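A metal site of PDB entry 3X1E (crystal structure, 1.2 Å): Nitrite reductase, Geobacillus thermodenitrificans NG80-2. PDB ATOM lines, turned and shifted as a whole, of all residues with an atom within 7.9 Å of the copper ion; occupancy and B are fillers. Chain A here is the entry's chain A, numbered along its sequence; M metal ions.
The backbone carbonyl oxygen (O) of Val 122 lies close to a ring nitrogen (NE2) of His 124 (3.4 Å). The backbone NH of Val 142 sits at hydrogen-bond distance from the backbone carbonyl oxygen of His 124 (2.7 Å). The backbone carbonyl oxygen (O) of Trp 92 lies close to the backbone NH (N) of Met 177. SG of Cys 164 lies close to OG1 of Thr 166. The backbone NH of His 124 sits close to the side-chain amide nitrogen of Asn 117, 3.5 Å away. The side-chain sulfur (SG) of Cys 164 lies close to the backbone NH (N) of Ser 125 (3.4 Å). A ring nitrogen (NE2) of His 124 sits at hydrogen-bond distance from the side-chain carboxylate (OD2) of Asp 119, 2.8 Å away.
Of the 27 residues printed, 4 come within 4 Å of the copper ion.
The copper ion is bound by a ring nitrogen (ND1) of His 172 (2.0 Å). The copper ion is bound by ND1 of His 124. SG of Cys 164 is bound to the copper ion (2.2 Å). The side-chain sulfur (SD) of Met 177 is bound to the copper ion (2.6 Å).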
ATOM      1  N   ALA A  76     -11.521 -10.670  -1.772  1.00  0.00           N
ATOM      2  CA  ALA A  76     -11.236 -11.714  -0.849  1.00  0.00           C
ATOM      3  C   ALA A  76     -11.996 -11.427   0.433  1.00  0.00           C
ATOM      4  O   ALA A  76     -11.931 -10.298   0.962  1.00  0.00           O
ATOM      5  CB  ALA A  76      -9.738 -11.802  -0.542  1.00  0.00           C
ATOM      6  N   TRP A  92     -12.644 -18.925   3.675  1.00  0.00           N
ATOM      7  CA  TRP A  92     -11.873 -17.868   2.986  1.00  0.00           C
ATOM      8  C   TRP A  92     -12.264 -17.924   1.527  1.00  0.00           C
ATOM      9  O   TRP A  92     -12.180 -19.003   0.924  1.00  0.00           O
ATOM     10  CB  TRP A  92     -10.381 -18.109   3.216  1.00  0.00           C
ATOM     11  CG  TRP A  92      -9.868 -18.112   4.589  1.00  0.00           C
ATOM     12  CD1 TRP A  92     -10.562 -18.157   5.785  1.00  0.00           C
ATOM     13  CD2 TRP A  92      -8.491 -18.198   4.946  1.00  0.00           C
ATOM     14  NE1 TRP A  92      -9.684 -18.198   6.836  1.00  0.00           N
ATOM     15  CE2 TRP A  92      -8.407 -18.243   6.351  1.00  0.00           C
ATOM     16  CE3 TRP A  92      -7.340 -18.308   4.211  1.00  0.00           C
ATOM     17  CZ2 TRP A  92      -7.203 -18.313   6.989  1.00  0.00           C
ATOM     18  CZ3 TRP A  92      -6.187 -18.384   4.899  1.00  0.00           C
ATOM     19  CH2 TRP A  92      -6.083 -18.351   6.242  1.00  0.00           C
ATOM     20  N   THR A  93     -12.725 -16.829   0.930  1.00  0.00           N
ATOM     21  CA  THR A  93     -13.418 -16.901  -0.343  1.00  0.00           C
ATOM     22  C   THR A  93     -12.996 -15.737  -1.236  1.00  0.00           C
ATOM     23  O   THR A  93     -12.529 -14.665  -0.759  1.00  0.00           O
ATOM     24  CB  THR A  93     -14.952 -16.827  -0.160  1.00  0.00           C
ATOM     25  OG1 THR A  93     -15.348 -15.466   0.119  1.00  0.00           O
ATOM     26  CG2 THR A  93     -15.488 -17.789   0.804  1.00  0.00           C
ATOM     27  N   PHE A  94     -13.257 -15.951  -2.520  1.00  0.00           N
ATOM     28  CA  PHE A  94     -13.463 -14.881  -3.480  1.00  0.00           C
ATOM     29  C   PHE A  94     -14.928 -14.580  -3.521  1.00  0.00           C
ATOM     30  O   PHE A  94     -15.720 -15.409  -3.884  1.00  0.00           O
ATOM     31  CB  PHE A  94     -12.881 -15.204  -4.828  1.00  0.00           C
ATOM     32  CG  PHE A  94     -11.407 -15.452  -4.810  1.00  0.00           C
ATOM     33  CD1 PHE A  94     -10.526 -14.395  -4.673  1.00  0.00           C
ATOM     34  CD2 PHE A  94     -10.856 -16.746  -4.848  1.00  0.00           C
ATOM     35  CE1 PHE A  94      -9.161 -14.616  -4.734  1.00  0.00           C
ATOM     36  CE2 PHE A  94      -9.501 -16.923  -4.944  1.00  0.00           C
ATOM     37  CZ  PHE A  94      -8.659 -15.873  -4.849  1.00  0.00           C
ATOM     38  N   LEU A 115      -8.042  -7.228  -7.098  1.00  0.00           N
ATOM     39  CA  LEU A 115      -8.466  -7.885  -5.877  1.00  0.00           C
ATOM     40  C   LEU A 115      -8.586  -6.861  -4.788  1.00  0.00           C
ATOM     41  O   LEU A 115      -7.630  -6.151  -4.508  1.00  0.00           O
ATOM     42  CB  LEU A 115      -7.512  -8.996  -5.508  1.00  0.00           C
ATOM     43  CG  LEU A 115      -7.844  -9.802  -4.294  1.00  0.00           C
ATOM     44  CD1 LEU A 115      -9.108 -10.635  -4.510  1.00  0.00           C
ATOM     45  CD2 LEU A 115      -6.705 -10.687  -3.847  1.00  0.00           C
ATOM     46  N   ASN A 117      -9.103  -6.804  -0.953  1.00  0.00           N
ATOM     47  CA  ASN A 117      -8.983  -7.693   0.176  1.00  0.00           C
ATOM     48  C   ASN A 117      -9.816  -7.156   1.365  1.00  0.00           C
ATOM     49  O   ASN A 117      -9.459  -6.185   2.010  1.00  0.00           O
ATOM     50  CB  ASN A 117      -7.534  -7.892   0.562  1.00  0.00           C
ATOM     51  CG  ASN A 117      -7.409  -8.974   1.629  1.00  0.00           C
ATOM     52  OD1 ASN A 117      -8.425  -9.552   2.048  1.00  0.00           O
ATOM     53  ND2 ASN A 117      -6.220  -9.215   2.078  1.00  0.00           N
ATOM     54  N   ASP A 119     -10.575  -9.172   3.990  1.00  0.00           N
ATOM     55  CA  ASP A 119     -10.168  -9.887   5.142  1.00  0.00           C
ATOM     56  C   ASP A 119      -9.495  -8.897   6.115  1.00  0.00           C
ATOM     57  O   ASP A 119      -8.632  -8.174   5.721  1.00  0.00           O
ATOM     58  CB  ASP A 119      -9.214 -11.025   4.753  1.00  0.00           C
ATOM     59  CG  ASP A 119      -8.873 -11.950   5.891  1.00  0.00           C
ATOM     60  OD1 ASP A 119      -8.685 -11.496   7.081  1.00  0.00           O
ATOM     61  OD2 ASP A 119      -8.730 -13.179   5.655  1.00  0.00           O
ATOM     62  N   VAL A 122      -5.739 -11.259   7.138  1.00  0.00           N
ATOM     63  CA  VAL A 122      -4.895 -12.129   6.315  1.00  0.00           C
ATOM     64  C   VAL A 122      -4.768 -11.512   4.946  1.00  0.00           C
ATOM     65  O   VAL A 122      -5.757 -11.108   4.327  1.00  0.00           O
ATOM     66  CB  VAL A 122      -5.510 -13.564   6.178  1.00  0.00           C
ATOM     67  CG1 VAL A 122      -4.498 -14.474   5.564  1.00  0.00           C
ATOM     68  CG2 VAL A 122      -5.879 -14.078   7.576  1.00  0.00           C
ATOM     69  N   PRO A 123      -3.502 -11.460   4.411  1.00  0.00           N
ATOM     70  CA  PRO A 123      -3.280 -11.117   2.993  1.00  0.00           C
ATOM     71  C   PRO A 123      -3.802 -12.190   2.063  1.00  0.00           C
ATOM     72  O   PRO A 123      -3.807 -13.342   2.377  1.00  0.00           O
ATOM     73  CB  PRO A 123      -1.751 -10.977   2.883  1.00  0.00           C
ATOM     74  CG  PRO A 123      -1.270 -10.865   4.300  1.00  0.00           C
ATOM     75  CD  PRO A 123      -2.235 -11.746   5.097  1.00  0.00           C
ATOM     76  N   HIS A 124      -4.185 -11.733   0.882  1.00  0.00           N
ATOM     77  CA  HIS A 124      -4.647 -12.702  -0.157  1.00  0.00           C
ATOM     78  C   HIS A 124      -4.168 -12.252  -1.500  1.00  0.00           C
ATOM     79  O   HIS A 124      -3.672 -11.175  -1.697  1.00  0.00           O
ATOM     80  CB  HIS A 124      -6.175 -12.796  -0.183  1.00  0.00           C
ATOM     81  CG  HIS A 124      -6.703 -13.317   1.152  1.00  0.00           C
ATOM     82  ND1 HIS A 124      -6.547 -14.624   1.531  1.00  0.00           N
ATOM     83  CD2 HIS A 124      -7.424 -12.744   2.134  1.00  0.00           C
ATOM     84  CE1 HIS A 124      -7.098 -14.824   2.701  1.00  0.00           C
ATOM     85  NE2 HIS A 124      -7.611 -13.692   3.114  1.00  0.00           N
ATOM     86  N   SER A 125      -4.271 -13.153  -2.467  1.00  0.00           N
ATOM     87  CA  SER A 125      -3.738 -12.953  -3.818  1.00  0.00           C
ATOM     88  C   SER A 125      -4.543 -13.765  -4.782  1.00  0.00           C
ATOM     89  O   SER A 125      -5.537 -14.427  -4.413  1.00  0.00           O
ATOM     90  CB  SER A 125      -2.281 -13.337  -3.846  1.00  0.00           C
ATOM     91  OG  SER A 125      -2.102 -14.747  -3.528  1.00  0.00           O
ATOM     92  N   MET A 126      -4.170 -13.628  -6.041  1.00  0.00           N
ATOM     93  CA  MET A 126      -4.865 -14.364  -7.136  1.00  0.00           C
ATOM     94  C   MET A 126      -3.883 -14.913  -8.194  1.00  0.00           C
ATOM     95  O   MET A 126      -2.998 -14.237  -8.703  1.00  0.00           O
ATOM     96  CB  MET A 126      -5.851 -13.485  -7.864  1.00  0.00           C
ATOM     97  CG  MET A 126      -6.476 -14.125  -9.079  1.00  0.00           C
ATOM     98  SD  MET A 126      -7.487 -15.581  -8.728  1.00  0.00           S
ATOM     99  CE  MET A 126      -9.016 -14.727  -8.327  1.00  0.00           C
ATOM    100  N   ASP A 141       0.714 -10.597  -2.945  1.00  0.00           N
ATOM    101  CA  ASP A 141      -0.242 -10.385  -1.925  1.00  0.00           C
ATOM    102  C   ASP A 141      -0.824  -8.994  -1.947  1.00  0.00           C
ATOM    103  O   ASP A 141      -0.136  -8.034  -2.236  1.00  0.00           O
ATOM    104  CB  ASP A 141       0.366 -10.682  -0.523  1.00  0.00           C
ATOM    105  CG  ASP A 141       0.667 -12.150  -0.302  1.00  0.00           C
ATOM    106  OD1 ASP A 141       0.160 -13.022  -1.048  1.00  0.00           O
ATOM    107  OD2 ASP A 141       1.419 -12.375   0.657  1.00  0.00           O
ATOM    108  N   VAL A 142      -2.089  -8.931  -1.631  1.00  0.00           N
ATOM    109  CA  VAL A 142      -2.833  -7.702  -1.301  1.00  0.00           C
ATOM    110  C   VAL A 142      -3.131  -7.711   0.174  1.00  0.00           C
ATOM    111  O   VAL A 142      -3.742  -8.687   0.713  1.00  0.00           O
ATOM    112  CB  VAL A 142      -4.104  -7.622  -2.221  1.00  0.00           C
ATOM    113  CG1 VAL A 142      -4.839  -6.333  -1.893  1.00  0.00           C
ATOM    114  CG2 VAL A 142      -3.865  -7.654  -3.701  1.00  0.00           C
ATOM    115  N   HIS A 163      -6.960 -19.604  -8.035  1.00  0.00           N
ATOM    116  CA  HIS A 163      -6.905 -19.744  -6.591  1.00  0.00           C
ATOM    117  C   HIS A 163      -6.029 -18.665  -6.018  1.00  0.00           C
ATOM    118  O   HIS A 163      -5.220 -18.103  -6.692  1.00  0.00           O
ATOM    119  CB  HIS A 163      -6.417 -21.125  -6.216  1.00  0.00           C
ATOM    120  CG  HIS A 163      -5.047 -21.422  -6.678  1.00  0.00           C
ATOM    121  ND1 HIS A 163      -3.890 -21.116  -5.988  1.00  0.00           N
ATOM    122  CD2 HIS A 163      -4.622 -22.085  -7.794  1.00  0.00           C
ATOM    123  CE1 HIS A 163      -2.814 -21.565  -6.671  1.00  0.00           C
ATOM    124  NE2 HIS A 163      -3.232 -22.115  -7.763  1.00  0.00           N
ATOM    125  N   CYS A 164      -6.179 -18.495  -4.673  1.00  0.00           N
ATOM    126  CA  CYS A 164      -5.241 -17.649  -3.904  1.00  0.00           C
ATOM    127  C   CYS A 164      -3.871 -18.291  -3.882  1.00  0.00           C
ATOM    128  O   CYS A 164      -3.752 -19.530  -3.767  1.00  0.00           O
ATOM    129  CB  CYS A 164      -5.792 -17.402  -2.504  1.00  0.00           C
ATOM    130  SG  CYS A 164      -4.700 -16.405  -1.526  1.00  0.00           S
ATOM    131  N   GLY A 165      -2.862 -17.457  -4.080  1.00  0.00           N
ATOM    132  CA  GLY A 165      -1.474 -17.878  -4.143  1.00  0.00           C
ATOM    133  C   GLY A 165      -0.615 -17.485  -2.933  1.00  0.00           C
ATOM    134  O   GLY A 165       0.586 -17.420  -3.054  1.00  0.00           O
ATOM    135  N   THR A 166      -1.254 -17.147  -1.815  1.00  0.00           N
ATOM    136  CA  THR A 166      -0.546 -16.642  -0.644  1.00  0.00           C
ATOM    137  C   THR A 166      -0.047 -17.823   0.195  1.00  0.00           C
ATOM    138  O   THR A 166      -0.765 -18.791   0.462  1.00  0.00           O
ATOM    139  CB  THR A 166      -1.511 -15.733   0.172  1.00  0.00           C
ATOM    140  OG1 THR A 166      -1.899 -14.636  -0.616  1.00  0.00           O
ATOM    141  CG2 THR A 166      -0.905 -15.211   1.454  1.00  0.00           C
ATOM    142  N   LYS A 167       1.216 -17.750   0.639  1.00  0.00           N
ATOM    143  CA  LYS A 167       1.794 -18.835   1.440  1.00  0.00           C
ATOM    144  C   LYS A 167       1.137 -18.822   2.843  1.00  0.00           C
ATOM    145  O   LYS A 167       0.972 -17.748   3.474  1.00  0.00           O
ATOM    146  CB  LYS A 167       3.340 -18.666   1.605  1.00  0.00           C
ATOM    147  CG  LYS A 167       4.075 -19.650   2.519  1.00  0.00           C
ATOM    148  CD  LYS A 167       5.528 -19.160   2.499  1.00  0.00           C
ATOM    149  CE  LYS A 167       6.613 -20.222   2.633  1.00  0.00           C
ATOM    150  NZ  LYS A 167       7.654 -20.065   1.564  1.00  0.00           N
ATOM    151  N   PRO A 168       0.810 -20.014   3.371  1.00  0.00           N
ATOM    152  CA  PRO A 168       0.899 -21.327   2.712  1.00  0.00           C
ATOM    153  C   PRO A 168      -0.267 -21.526   1.782  1.00  0.00           C
ATOM    154  O   PRO A 168      -1.444 -21.424   2.214  1.00  0.00           O
ATOM    155  CB  PRO A 168       0.831 -22.316   3.899  1.00  0.00           C
ATOM    156  CG  PRO A 168       0.772 -21.476   5.109  1.00  0.00           C
ATOM    157  CD  PRO A 168       0.305 -20.137   4.761  1.00  0.00           C
ATOM    158  N   VAL A 169       0.043 -21.806   0.547  1.00  0.00           N
ATOM    159  CA  VAL A 169      -1.013 -21.921  -0.483  1.00  0.00           C
ATOM    160  C   VAL A 169      -2.030 -23.015  -0.123  1.00  0.00           C
ATOM    161  O   VAL A 169      -3.231 -22.834  -0.316  1.00  0.00           O
ATOM    162  CB  VAL A 169      -0.433 -22.097  -1.886  1.00  0.00           C
ATOM    163  CG1 VAL A 169      -1.496 -22.415  -2.898  1.00  0.00           C
ATOM    164  CG2 VAL A 169       0.393 -20.888  -2.306  1.00  0.00           C
ATOM    165  N   GLN A 171      -3.193 -23.745   2.722  1.00  0.00           N
ATOM    166  CA  GLN A 171      -4.134 -23.205   3.688  1.00  0.00           C
ATOM    167  C   GLN A 171      -5.179 -22.360   2.987  1.00  0.00           C
ATOM    168  O   GLN A 171      -6.401 -22.463   3.264  1.00  0.00           O
ATOM    169  CB  GLN A 171      -3.349 -22.425   4.759  1.00  0.00           C
ATOM    170  CG  GLN A 171      -4.240 -21.903   5.804  1.00  0.00           C
ATOM    171  CD  GLN A 171      -3.465 -21.165   6.891  1.00  0.00           C
ATOM    172  OE1 GLN A 171      -2.319 -20.772   6.705  1.00  0.00           O
ATOM    173  NE2 GLN A 171      -4.072 -20.998   8.010  1.00  0.00           N
ATOM    174  N   HIS A 172      -4.711 -21.504   2.061  1.00  0.00           N
ATOM    175  CA  HIS A 172      -5.638 -20.590   1.388  1.00  0.00           C
ATOM    176  C   HIS A 172      -6.594 -21.356   0.438  1.00  0.00           C
ATOM    177  O   HIS A 172      -7.809 -21.105   0.433  1.00  0.00           O
ATOM    178  CB  HIS A 172      -4.836 -19.551   0.677  1.00  0.00           C
ATOM    179  CG  HIS A 172      -4.244 -18.550   1.630  1.00  0.00           C
ATOM    180  ND1 HIS A 172      -4.766 -17.265   1.758  1.00  0.00           N
ATOM    181  CD2 HIS A 172      -3.213 -18.637   2.487  1.00  0.00           C
ATOM    182  CE1 HIS A 172      -4.048 -16.632   2.692  1.00  0.00           C
ATOM    183  NE2 HIS A 172      -3.080 -17.426   3.106  1.00  0.00           N
ATOM    184  N   ILE A 173      -6.060 -22.345  -0.271  1.00  0.00           N
ATOM    185  CA  ILE A 173      -6.916 -23.182  -1.108  1.00  0.00           C
ATOM    186  C   ILE A 173      -7.874 -23.949  -0.247  1.00  0.00           C
ATOM    187  O   ILE A 173      -9.112 -23.923  -0.499  1.00  0.00           O
ATOM    188  CB  ILE A 173      -6.130 -24.099  -2.057  1.00  0.00           C
ATOM    189  CG1 ILE A 173      -5.221 -23.291  -3.024  1.00  0.00           C
ATOM    190  CG2 ILE A 173      -7.096 -24.998  -2.812  1.00  0.00           C
ATOM    191  CD1 ILE A 173      -4.415 -24.142  -4.027  1.00  0.00           C
ATOM    192  N   ASN A 175      -9.086 -23.524   2.615  1.00  0.00           N
ATOM    193  CA  ASN A 175     -10.127 -22.741   3.275  1.00  0.00           C
ATOM    194  C   ASN A 175     -11.166 -22.152   2.344  1.00  0.00           C
ATOM    195  O   ASN A 175     -12.140 -21.619   2.826  1.00  0.00           O
ATOM    196  CB  ASN A 175      -9.545 -21.625   4.100  1.00  0.00           C
ATOM    197  CG  ASN A 175      -9.004 -22.110   5.470  1.00  0.00           C
ATOM    198  OD1 ASN A 175      -9.537 -23.019   6.138  1.00  0.00           O
ATOM    199  ND2 ASN A 175      -7.929 -21.488   5.923  1.00  0.00           N
ATOM    200  N   GLY A 176     -10.977 -22.346   1.046  1.00  0.00           N
ATOM    201  CA  GLY A 176     -12.000 -22.009   0.027  1.00  0.00           C
ATOM    202  C   GLY A 176     -11.639 -21.186  -1.165  1.00  0.00           C
ATOM    203  O   GLY A 176     -12.514 -20.912  -1.949  1.00  0.00           O
ATOM    204  N   MET A 177     -10.385 -20.742  -1.244  1.00  0.00           N
ATOM    205  CA  MET A 177     -10.019 -19.753  -2.206  1.00  0.00           C
ATOM    206  C   MET A 177      -9.542 -20.392  -3.531  1.00  0.00           C
ATOM    207  O   MET A 177      -8.387 -20.441  -3.906  1.00  0.00           O
ATOM    208  CB  MET A 177      -8.910 -18.869  -1.654  1.00  0.00           C
ATOM    209  CG  MET A 177      -9.365 -18.175  -0.464  1.00  0.00           C
ATOM    210  SD  MET A 177      -8.366 -16.770   0.186  1.00  0.00           S
ATOM    211  CE  MET A 177      -9.022 -15.574  -0.905  1.00  0.00           C
HETATM  212 CU    CU M   1      -5.797 -16.205   0.397  1.00  0.00          CU
